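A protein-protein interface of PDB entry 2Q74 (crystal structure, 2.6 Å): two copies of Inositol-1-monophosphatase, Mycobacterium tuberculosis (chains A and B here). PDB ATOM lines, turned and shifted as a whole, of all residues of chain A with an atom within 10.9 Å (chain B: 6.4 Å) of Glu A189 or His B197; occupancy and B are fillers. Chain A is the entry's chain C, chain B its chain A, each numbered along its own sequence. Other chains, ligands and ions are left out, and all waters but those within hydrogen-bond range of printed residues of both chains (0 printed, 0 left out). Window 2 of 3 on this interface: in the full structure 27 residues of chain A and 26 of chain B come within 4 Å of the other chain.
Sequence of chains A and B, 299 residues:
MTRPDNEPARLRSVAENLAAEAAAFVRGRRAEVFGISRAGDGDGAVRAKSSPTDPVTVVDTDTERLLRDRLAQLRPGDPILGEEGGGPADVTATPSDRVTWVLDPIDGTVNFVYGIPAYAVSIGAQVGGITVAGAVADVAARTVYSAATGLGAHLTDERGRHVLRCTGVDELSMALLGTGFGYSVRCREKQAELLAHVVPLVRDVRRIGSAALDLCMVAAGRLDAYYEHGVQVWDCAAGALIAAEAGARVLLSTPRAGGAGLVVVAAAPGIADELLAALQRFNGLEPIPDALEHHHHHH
Among the printed residues, merely in contact across the chains: Phe A181 with Val B199, Arg A188 with Val B199, Glu A189 with Ala B196, Glu A189 with His B197, Glu A189 with Pro B200, Ala A192 with Ala B196, Ala A192 with Val B199, Glu A193 with Ala B196, Ala A196 with Ala B192 and Ala A196 with Glu B193.
The side-chain carboxylate (OE2) of Glu A193 lies close to the side-chain carboxylate (OE2) of Glu B193 (3.3 Å).
Glu A189 touches three residues of chain B.
His B197 touches just one residue of chain A: Glu A189 (3.4 Å).
Ala B196 touches just these residues of chain A: Glu A189 (2.9 Å), Ala A192 (3.3 Å) and Glu A193 (3.6 Å).
No residue of chain A comes within 4 Å of Val B198.
Of the printed residues of chain A, Pro B200 touches Glu A189 (3.8 Å).
No residue of chain A comes within 4 Å of Phe B282.
Of the printed residues of chain B, Arg A188 touches Val B199 (3.8 Å).
Of the printed residues of chain B, Ala A192 touches Ala B196 (3.3 Å) and Val B199 (3.8 Å).
Printed residues of chain B within 4 Å of Glu A193: Glu B193 (3.3 Å) and Ala B196 (3.6 Å).
Of the printed residues of chain A, Glu B193 touches Glu A193 (3.3 Å) and Ala A196 (3.7 Å).
Lys A190 touches none of the printed residues of chain B.
Leu A194 touches none of the printed residues of chain B.
The nearest residue of chain A that does not touch His B197 is Glu A193 (4.3 Å).
Hydrophobic or aromatic side chains of chain A within 4 Å of the printed part of chain B: Phe A181, Ala A192 and Ala A196.
Printed residues of chain B that touch a printed residue of chain A: Ala B192, Glu B193, Ala B196, His B197, Val B199 and Pro B200.
Hydrophobic or aromatic side chains of chain B that line the printed part of chain A: Ala B192, Ala B196, His B197, Val B199 and Pro B200.
Among the printed residues, 11 pairs touch across the chains.
Among the printed residues, no Asp or Glu carboxylate lies within 4 Å of a Lys or Arg side-chain nitrogen of the other chain.
Ala A192 touches Ala B196, and with the chains exchanged Ala A196 touches Ala B192.
Glu A193 touches its own counterpart, Glu B193.
Glu A193 touches Ala B196, and with the chains exchanged Ala A196 touches Glu B193.
Of the 11 pairs that touch across the chains among the printed residues, 5 have their exchanged pair printed and touching as well.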
ATOM      1  N   GLY A 180      -4.580  -6.588 -30.468  1.00  0.00           N
ATOM      2  CA  GLY A 180      -4.685  -7.475 -29.327  1.00  0.00           C
ATOM      3  C   GLY A 180      -3.460  -7.304 -28.459  1.00  0.00           C
ATOM      4  O   GLY A 180      -2.584  -6.498 -28.758  1.00  0.00           O
ATOM      5  N   PHE A 181      -3.397  -8.071 -27.385  1.00  0.00           N
ATOM      6  CA  PHE A 181      -2.177  -8.211 -26.611  1.00  0.00           C
ATOM      7  C   PHE A 181      -1.709  -9.655 -26.736  1.00  0.00           C
ATOM      8  O   PHE A 181      -2.529 -10.595 -26.658  1.00  0.00           O
ATOM      9  CB  PHE A 181      -2.414  -7.868 -25.145  1.00  0.00           C
ATOM     10  CG  PHE A 181      -2.824  -6.428 -24.902  1.00  0.00           C
ATOM     11  CD1 PHE A 181      -3.875  -6.134 -24.036  1.00  0.00           C
ATOM     12  CD2 PHE A 181      -2.171  -5.373 -25.539  1.00  0.00           C
ATOM     13  CE1 PHE A 181      -4.260  -4.831 -23.806  1.00  0.00           C
ATOM     14  CE2 PHE A 181      -2.547  -4.065 -25.306  1.00  0.00           C
ATOM     15  CZ  PHE A 181      -3.588  -3.791 -24.423  1.00  0.00           C
ATOM     16  N   GLY A 182      -0.399  -9.829 -26.931  1.00  0.00           N
ATOM     17  CA  GLY A 182       0.186 -11.156 -27.104  1.00  0.00           C
ATOM     18  C   GLY A 182       0.959 -11.710 -25.910  1.00  0.00           C
ATOM     19  O   GLY A 182       2.010 -11.170 -25.544  1.00  0.00           O
ATOM     20  N   TYR A 183       0.460 -12.802 -25.322  1.00  0.00           N
ATOM     21  CA  TYR A 183       1.130 -13.490 -24.186  1.00  0.00           C
ATOM     22  C   TYR A 183       0.163 -14.436 -23.482  1.00  0.00           C
ATOM     23  O   TYR A 183      -1.040 -14.164 -23.405  1.00  0.00           O
ATOM     24  CB  TYR A 183       1.710 -12.489 -23.173  1.00  0.00           C
ATOM     25  N   ARG A 186       2.352 -10.018 -19.118  1.00  0.00           N
ATOM     26  CA  ARG A 186       3.477  -9.171 -18.703  1.00  0.00           C
ATOM     27  C   ARG A 186       3.635  -7.972 -19.641  1.00  0.00           C
ATOM     28  O   ARG A 186       3.608  -8.124 -20.879  1.00  0.00           O
ATOM     29  CB  ARG A 186       4.787  -9.971 -18.669  1.00  0.00           C
ATOM     30  N   CYS A 187       3.781  -6.784 -19.045  1.00  0.00           N
ATOM     31  CA  CYS A 187       4.067  -5.541 -19.781  1.00  0.00           C
ATOM     32  C   CYS A 187       2.890  -4.871 -20.546  1.00  0.00           C
ATOM     33  O   CYS A 187       3.080  -3.853 -21.221  1.00  0.00           O
ATOM     34  CB  CYS A 187       5.268  -5.753 -20.712  1.00  0.00           C
ATOM     35  SG  CYS A 187       5.084  -5.066 -22.381  1.00  0.00           S
ATOM     36  N   ARG A 188       1.687  -5.421 -20.423  1.00  0.00           N
ATOM     37  CA  ARG A 188       0.508  -4.953 -21.168  1.00  0.00           C
ATOM     38  C   ARG A 188       0.289  -3.433 -21.234  1.00  0.00           C
ATOM     39  O   ARG A 188      -0.096  -2.910 -22.293  1.00  0.00           O
ATOM     40  CB  ARG A 188      -0.746  -5.629 -20.612  1.00  0.00           C
ATOM     41  CG  ARG A 188      -0.915  -7.043 -21.109  1.00  0.00           C
ATOM     42  CD  ARG A 188      -2.297  -7.572 -20.823  1.00  0.00           C
ATOM     43  NE  ARG A 188      -2.505  -8.870 -21.460  1.00  0.00           N
ATOM     44  CZ  ARG A 188      -3.639  -9.562 -21.401  1.00  0.00           C
ATOM     45  NH1 ARG A 188      -4.681  -9.084 -20.718  1.00  0.00           N
ATOM     46  NH2 ARG A 188      -3.738 -10.742 -22.019  1.00  0.00           N
ATOM     47  N   GLU A 189       0.527  -2.737 -20.121  1.00  0.00           N
ATOM     48  CA  GLU A 189       0.282  -1.292 -20.054  1.00  0.00           C
ATOM     49  C   GLU A 189       1.067  -0.487 -21.102  1.00  0.00           C
ATOM     50  O   GLU A 189       0.553   0.505 -21.620  1.00  0.00           O
ATOM     51  CB  GLU A 189       0.558  -0.734 -18.652  1.00  0.00           C
ATOM     52  CG  GLU A 189      -0.240   0.524 -18.376  1.00  0.00           C
ATOM     53  CD  GLU A 189       0.174   1.264 -17.126  1.00  0.00           C
ATOM     54  OE1 GLU A 189       0.558   0.620 -16.125  1.00  0.00           O
ATOM     55  OE2 GLU A 189       0.085   2.510 -17.137  1.00  0.00           O
ATOM     56  N   LYS A 190       2.288  -0.918 -21.418  1.00  0.00           N
ATOM     57  CA  LYS A 190       3.086  -0.291 -22.480  1.00  0.00           C
ATOM     58  C   LYS A 190       2.436  -0.425 -23.862  1.00  0.00           C
ATOM     59  O   LYS A 190       2.430   0.525 -24.648  1.00  0.00           O
ATOM     60  CB  LYS A 190       4.478  -0.918 -22.561  1.00  0.00           C
ATOM     61  CG  LYS A 190       5.345  -0.719 -21.345  1.00  0.00           C
ATOM     62  CD  LYS A 190       6.665  -1.481 -21.499  1.00  0.00           C
ATOM     63  CE  LYS A 190       7.434  -1.571 -20.173  1.00  0.00           C
ATOM     64  NZ  LYS A 190       8.761  -2.243 -20.303  1.00  0.00           N
ATOM     65  N   GLN A 191       1.915  -1.615 -24.162  1.00  0.00           N
ATOM     66  CA  GLN A 191       1.223  -1.852 -25.429  1.00  0.00           C
ATOM     67  C   GLN A 191       0.011  -0.941 -25.529  1.00  0.00           C
ATOM     68  O   GLN A 191      -0.264  -0.400 -26.593  1.00  0.00           O
ATOM     69  CB  GLN A 191       0.755  -3.302 -25.551  1.00  0.00           C
ATOM     70  CG  GLN A 191       1.848  -4.363 -25.518  1.00  0.00           C
ATOM     71  CD  GLN A 191       1.281  -5.786 -25.502  1.00  0.00           C
ATOM     72  OE1 GLN A 191       0.642  -6.234 -26.465  1.00  0.00           O
ATOM     73  NE2 GLN A 191       1.515  -6.501 -24.403  1.00  0.00           N
ATOM     74  N   ALA A 192      -0.705  -0.791 -24.415  1.00  0.00           N
ATOM     75  CA  ALA A 192      -1.890   0.065 -24.335  1.00  0.00           C
ATOM     76  C   ALA A 192      -1.507   1.525 -24.495  1.00  0.00           C
ATOM     77  O   ALA A 192      -2.214   2.315 -25.128  1.00  0.00           O
ATOM     78  CB  ALA A 192      -2.596  -0.148 -23.000  1.00  0.00           C
ATOM     79  N   GLU A 193      -0.381   1.871 -23.892  1.00  0.00           N
ATOM     80  CA  GLU A 193       0.167   3.215 -23.963  1.00  0.00           C
ATOM     81  C   GLU A 193       0.474   3.540 -25.420  1.00  0.00           C
ATOM     82  O   GLU A 193       0.091   4.584 -25.933  1.00  0.00           O
ATOM     83  CB  GLU A 193       1.447   3.283 -23.124  1.00  0.00           C
ATOM     84  CG  GLU A 193       1.722   4.614 -22.454  1.00  0.00           C
ATOM     85  CD  GLU A 193       1.027   4.751 -21.108  1.00  0.00           C
ATOM     86  OE1 GLU A 193       1.148   3.830 -20.260  1.00  0.00           O
ATOM     87  OE2 GLU A 193       0.372   5.797 -20.894  1.00  0.00           O
ATOM     88  N   LEU A 194       1.154   2.609 -26.079  1.00  0.00           N
ATOM     89  CA  LEU A 194       1.466   2.723 -27.496  1.00  0.00           C
ATOM     90  C   LEU A 194       0.216   2.939 -28.349  1.00  0.00           C
ATOM     91  O   LEU A 194       0.227   3.755 -29.274  1.00  0.00           O
ATOM     92  CB  LEU A 194       2.193   1.468 -27.983  1.00  0.00           C
ATOM     93  CG  LEU A 194       2.432   1.331 -29.496  1.00  0.00           C
ATOM     94  CD1 LEU A 194       3.571   2.222 -29.945  1.00  0.00           C
ATOM     95  CD2 LEU A 194       2.715  -0.121 -29.843  1.00  0.00           C
ATOM     96  N   LEU A 195      -0.847   2.195 -28.055  1.00  0.00           N
ATOM     97  CA  LEU A 195      -2.070   2.273 -28.848  1.00  0.00           C
ATOM     98  C   LEU A 195      -2.762   3.611 -28.701  1.00  0.00           C
ATOM     99  O   LEU A 195      -3.305   4.140 -29.663  1.00  0.00           O
ATOM    100  CB  LEU A 195      -3.036   1.142 -28.484  1.00  0.00           C
ATOM    101  CG  LEU A 195      -2.624  -0.263 -28.954  1.00  0.00           C
ATOM    102  CD1 LEU A 195      -3.735  -1.282 -28.621  1.00  0.00           C
ATOM    103  CD2 LEU A 195      -2.262  -0.310 -30.440  1.00  0.00           C
ATOM    104  N   ALA A 196      -2.746   4.154 -27.493  1.00  0.00           N
ATOM    105  CA  ALA A 196      -3.332   5.462 -27.253  1.00  0.00           C
ATOM    106  C   ALA A 196      -2.726   6.491 -28.198  1.00  0.00           C
ATOM    107  O   ALA A 196      -3.425   7.359 -28.694  1.00  0.00           O
ATOM    108  CB  ALA A 196      -3.159   5.877 -25.800  1.00  0.00           C
ATOM    109  N   HIS A 197      -1.437   6.357 -28.485  1.00  0.00           N
ATOM    110  CA  HIS A 197      -0.772   7.253 -29.430  1.00  0.00           C
ATOM    111  C   HIS A 197      -1.260   7.104 -30.877  1.00  0.00           C
ATOM    112  O   HIS A 197      -1.380   8.090 -31.595  1.00  0.00           O
ATOM    113  CB  HIS A 197       0.741   7.057 -29.389  1.00  0.00           C
ATOM    114  CG  HIS A 197       1.372   7.462 -28.095  1.00  0.00           C
ATOM    115  ND1 HIS A 197       2.709   7.275 -27.837  1.00  0.00           N
ATOM    116  CD2 HIS A 197       0.851   8.035 -26.985  1.00  0.00           C
ATOM    117  CE1 HIS A 197       2.990   7.722 -26.627  1.00  0.00           C
ATOM    118  NE2 HIS A 197       1.878   8.185 -26.086  1.00  0.00           N
ATOM    119  N   ARG A 207     -10.959  -4.522 -30.823  1.00  0.00           N
ATOM    120  CA  ARG A 207     -10.245  -5.518 -30.035  1.00  0.00           C
ATOM    121  C   ARG A 207     -11.150  -6.727 -29.782  1.00  0.00           C
ATOM    122  O   ARG A 207     -12.007  -6.720 -28.889  1.00  0.00           O
ATOM    123  CB  ARG A 207      -9.759  -4.875 -28.740  1.00  0.00           C
ATOM    124  CG  ARG A 207      -9.241  -5.805 -27.602  1.00  0.00           C
ATOM    125  CD  ARG A 207      -7.848  -6.328 -27.867  1.00  0.00           C
ATOM    126  NE  ARG A 207      -6.668  -5.573 -27.368  1.00  0.00           N
ATOM    127  CZ  ARG A 207      -6.569  -4.271 -27.053  1.00  0.00           C
ATOM    128  NH1 ARG A 207      -7.586  -3.421 -27.093  1.00  0.00           N
ATOM    129  NH2 ARG A 207      -5.392  -3.802 -26.667  1.00  0.00           N
ATOM    130  N   TYR A 227      -2.612  -4.970 -35.918  1.00  0.00           N
ATOM    131  CA  TYR A 227      -1.324  -4.890 -35.248  1.00  0.00           C
ATOM    132  C   TYR A 227      -1.368  -5.579 -33.893  1.00  0.00           C
ATOM    133  O   TYR A 227      -2.205  -5.243 -33.028  1.00  0.00           O
ATOM    134  CB  TYR A 227      -0.910  -3.425 -35.054  1.00  0.00           C
ATOM    135  CG  TYR A 227       0.161  -3.242 -34.004  1.00  0.00           C
ATOM    136  CD1 TYR A 227       1.459  -3.700 -34.230  1.00  0.00           C
ATOM    137  CD2 TYR A 227      -0.125  -2.641 -32.776  1.00  0.00           C
ATOM    138  CE1 TYR A 227       2.461  -3.558 -33.277  1.00  0.00           C
ATOM    139  CE2 TYR A 227       0.862  -2.489 -31.805  1.00  0.00           C
ATOM    140  CZ  TYR A 227       2.175  -2.950 -32.067  1.00  0.00           C
ATOM    141  OH  TYR A 227       3.215  -2.835 -31.144  1.00  0.00           O
ATOM    142  N   HIS A 229       1.570  -7.174 -30.832  1.00  0.00           N
ATOM    143  CA  HIS A 229       2.926  -7.422 -30.329  1.00  0.00           C
ATOM    144  C   HIS A 229       2.937  -8.649 -29.423  1.00  0.00           C
ATOM    145  O   HIS A 229       2.412  -8.605 -28.309  1.00  0.00           O
ATOM    146  CB  HIS A 229       3.420  -6.189 -29.557  1.00  0.00           C
ATOM    147  CG  HIS A 229       4.872  -6.241 -29.200  1.00  0.00           C
ATOM    148  ND1 HIS A 229       5.873  -5.947 -30.101  1.00  0.00           N
ATOM    149  CD2 HIS A 229       5.491  -6.553 -28.035  1.00  0.00           C
ATOM    150  CE1 HIS A 229       7.045  -6.083 -29.510  1.00  0.00           C
ATOM    151  NE2 HIS A 229       6.842  -6.445 -28.256  1.00  0.00           N
ATOM    152  N   PHE A 282       6.614   5.390 -32.345  1.00  0.00           N
ATOM    153  CA  PHE A 282       6.356   5.160 -30.925  1.00  0.00           C
ATOM    154  C   PHE A 282       6.933   3.844 -30.390  1.00  0.00           C
ATOM    155  O   PHE A 282       6.665   3.487 -29.253  1.00  0.00           O
ATOM    156  CB  PHE A 282       4.850   5.168 -30.660  1.00  0.00           C
ATOM    157  CG  PHE A 282       4.149   6.404 -31.140  1.00  0.00           C
ATOM    158  CD1 PHE A 282       3.030   6.306 -31.958  1.00  0.00           C
ATOM    159  CD2 PHE A 282       4.592   7.668 -30.767  1.00  0.00           C
ATOM    160  CE1 PHE A 282       2.370   7.454 -32.403  1.00  0.00           C
ATOM    161  CE2 PHE A 282       3.935   8.819 -31.205  1.00  0.00           C
ATOM    162  CZ  PHE A 282       2.829   8.714 -32.022  1.00  0.00           C
ATOM    163  N   ASN A 283       7.707   3.122 -31.198  1.00  0.00           N
ATOM    164  CA  ASN A 283       8.264   1.812 -30.812  1.00  0.00           C
ATOM    165  C   ASN A 283       7.235   0.705 -30.578  1.00  0.00           C
ATOM    166  O   ASN A 283       6.844   0.439 -29.434  1.00  0.00           O
ATOM    167  CB  ASN A 283       9.163   1.928 -29.573  1.00  0.00           C
ATOM    168  CG  ASN A 283      10.620   2.079 -29.928  1.00  0.00           C
ATOM    169  OD1 ASN A 283      11.493   1.868 -29.087  1.00  0.00           O
ATOM    170  ND2 ASN A 283      10.900   2.437 -31.177  1.00  0.00           N
ATOM    171  N   ALA B 192      -7.973   6.692 -24.358  1.00  0.00           N
ATOM    172  CA  ALA B 192      -7.038   5.592 -24.602  1.00  0.00           C
ATOM    173  C   ALA B 192      -5.953   5.548 -23.534  1.00  0.00           C
ATOM    174  O   ALA B 192      -5.543   4.482 -23.076  1.00  0.00           O
ATOM    175  CB  ALA B 192      -6.420   5.729 -25.982  1.00  0.00           C
ATOM    176  N   GLU B 193      -5.512   6.731 -23.143  1.00  0.00           N
ATOM    177  CA  GLU B 193      -4.512   6.910 -22.098  1.00  0.00           C
ATOM    178  C   GLU B 193      -5.053   6.360 -20.780  1.00  0.00           C
ATOM    179  O   GLU B 193      -4.370   5.624 -20.066  1.00  0.00           O
ATOM    180  CB  GLU B 193      -4.198   8.405 -21.947  1.00  0.00           C
ATOM    181  CG  GLU B 193      -2.769   8.743 -21.564  1.00  0.00           C
ATOM    182  CD  GLU B 193      -1.841   8.846 -22.771  1.00  0.00           C
ATOM    183  OE1 GLU B 193      -2.209   9.534 -23.758  1.00  0.00           O
ATOM    184  OE2 GLU B 193      -0.735   8.247 -22.725  1.00  0.00           O
ATOM    185  N   LEU B 194      -6.288   6.734 -20.467  1.00  0.00           N
ATOM    186  CA  LEU B 194      -6.980   6.232 -19.291  1.00  0.00           C
ATOM    187  C   LEU B 194      -7.067   4.715 -19.283  1.00  0.00           C
ATOM    188  O   LEU B 194      -6.845   4.092 -18.251  1.00  0.00           O
ATOM    189  CB  LEU B 194      -8.395   6.812 -19.227  1.00  0.00           C
ATOM    190  CG  LEU B 194      -9.338   6.263 -18.147  1.00  0.00           C
ATOM    191  CD1 LEU B 194      -9.014   6.842 -16.800  1.00  0.00           C
ATOM    192  CD2 LEU B 194     -10.767   6.568 -18.517  1.00  0.00           C
ATOM    193  N   LEU B 195      -7.406   4.126 -20.426  1.00  0.00           N
ATOM    194  CA  LEU B 195      -7.560   2.684 -20.522  1.00  0.00           C
ATOM    195  C   LEU B 195      -6.262   1.950 -20.295  1.00  0.00           C
ATOM    196  O   LEU B 195      -6.247   0.916 -19.643  1.00  0.00           O
ATOM    197  CB  LEU B 195      -8.142   2.270 -21.880  1.00  0.00           C
ATOM    198  CG  LEU B 195      -9.622   2.607 -22.085  1.00  0.00           C
ATOM    199  CD1 LEU B 195     -10.146   2.130 -23.455  1.00  0.00           C
ATOM    200  CD2 LEU B 195     -10.474   2.035 -20.932  1.00  0.00           C
ATOM    201  N   ALA B 196      -5.171   2.472 -20.843  1.00  0.00           N
ATOM    202  CA  ALA B 196      -3.868   1.865 -20.635  1.00  0.00           C
ATOM    203  C   ALA B 196      -3.625   1.684 -19.132  1.00  0.00           C
ATOM    204  O   ALA B 196      -3.114   0.665 -18.709  1.00  0.00           O
ATOM    205  CB  ALA B 196      -2.781   2.687 -21.287  1.00  0.00           C
ATOM    206  N   HIS B 197      -4.060   2.633 -18.323  1.00  0.00           N
ATOM    207  CA  HIS B 197      -3.896   2.518 -16.880  1.00  0.00           C
ATOM    208  C   HIS B 197      -4.710   1.385 -16.265  1.00  0.00           C
ATOM    209  O   HIS B 197      -4.249   0.724 -15.338  1.00  0.00           O
ATOM    210  CB  HIS B 197      -4.250   3.833 -16.179  1.00  0.00           C
ATOM    211  CG  HIS B 197      -3.320   4.965 -16.500  1.00  0.00           C
ATOM    212  ND1 HIS B 197      -3.532   6.248 -16.044  1.00  0.00           N
ATOM    213  CD2 HIS B 197      -2.189   5.012 -17.243  1.00  0.00           C
ATOM    214  CE1 HIS B 197      -2.565   7.034 -16.479  1.00  0.00           C
ATOM    215  NE2 HIS B 197      -1.739   6.309 -17.212  1.00  0.00           N
ATOM    216  N   VAL B 198      -5.922   1.163 -16.758  1.00  0.00           N
ATOM    217  CA  VAL B 198      -6.779   0.101 -16.211  1.00  0.00           C
ATOM    218  C   VAL B 198      -6.469  -1.282 -16.803  1.00  0.00           C
ATOM    219  O   VAL B 198      -6.750  -2.303 -16.175  1.00  0.00           O
ATOM    220  CB  VAL B 198      -8.297   0.468 -16.299  1.00  0.00           C
ATOM    221  CG1 VAL B 198      -8.560   1.529 -17.334  1.00  0.00           C
ATOM    222  CG2 VAL B 198      -9.150  -0.751 -16.547  1.00  0.00           C
ATOM    223  N   VAL B 199      -5.840  -1.304 -17.974  1.00  0.00           N
ATOM    224  CA  VAL B 199      -5.475  -2.552 -18.676  1.00  0.00           C
ATOM    225  C   VAL B 199      -4.759  -3.601 -17.799  1.00  0.00           C
ATOM    226  O   VAL B 199      -5.112  -4.773 -17.812  1.00  0.00           O
ATOM    227  CB  VAL B 199      -4.600  -2.262 -19.955  1.00  0.00           C
ATOM    228  CG1 VAL B 199      -3.868  -3.527 -20.438  1.00  0.00           C
ATOM    229  CG2 VAL B 199      -5.449  -1.676 -21.085  1.00  0.00           C
ATOM    230  N   PRO B 200      -3.740  -3.195 -17.043  1.00  0.00           N
ATOM    231  CA  PRO B 200      -3.087  -4.179 -16.176  1.00  0.00           C
ATOM    232  C   PRO B 200      -3.885  -4.595 -14.937  1.00  0.00           C
ATOM    233  O   PRO B 200      -3.540  -5.577 -14.301  1.00  0.00           O
ATOM    234  CB  PRO B 200      -1.802  -3.462 -15.754  1.00  0.00           C
ATOM    235  CG  PRO B 200      -2.169  -2.032 -15.778  1.00  0.00           C
ATOM    236  CD  PRO B 200      -3.089  -1.878 -16.949  1.00  0.00           C
ATOM    237  N   LEU B 201      -4.939  -3.869 -14.599  1.00  0.00           N
ATOM    238  CA  LEU B 201      -5.763  -4.228 -13.447  1.00  0.00           C
ATOM    239  C   LEU B 201      -6.842  -5.242 -13.790  1.00  0.00           C
ATOM    240  O   LEU B 201      -7.568  -5.670 -12.880  1.00  0.00           O
ATOM    241  CB  LEU B 201      -6.454  -2.994 -12.885  1.00  0.00           C
ATOM    242  CG  LEU B 201      -5.539  -1.909 -12.341  1.00  0.00           C
ATOM    243  CD1 LEU B 201      -6.376  -0.694 -12.013  1.00  0.00           C
ATOM    244  CD2 LEU B 201      -4.792  -2.404 -11.119  1.00  0.00           C
ATOM    245  N   PHE B 282      -8.060   7.474 -11.930  1.00  0.00           N
ATOM    246  CA  PHE B 282      -7.461   8.050 -13.138  1.00  0.00           C
ATOM    247  C   PHE B 282      -8.361   9.051 -13.877  1.00  0.00           C
ATOM    248  O   PHE B 282      -8.015   9.491 -14.970  1.00  0.00           O
ATOM    249  CB  PHE B 282      -7.091   6.934 -14.118  1.00  0.00           C
ATOM    250  CG  PHE B 282      -6.205   5.872 -13.538  1.00  0.00           C
ATOM    251  CD1 PHE B 282      -6.551   4.532 -13.641  1.00  0.00           C
ATOM    252  CD2 PHE B 282      -5.022   6.201 -12.908  1.00  0.00           C
ATOM    253  CE1 PHE B 282      -5.732   3.540 -13.113  1.00  0.00           C
ATOM    254  CE2 PHE B 282      -4.202   5.209 -12.382  1.00  0.00           C
ATOM    255  CZ  PHE B 282      -4.563   3.880 -12.482  1.00  0.00           C
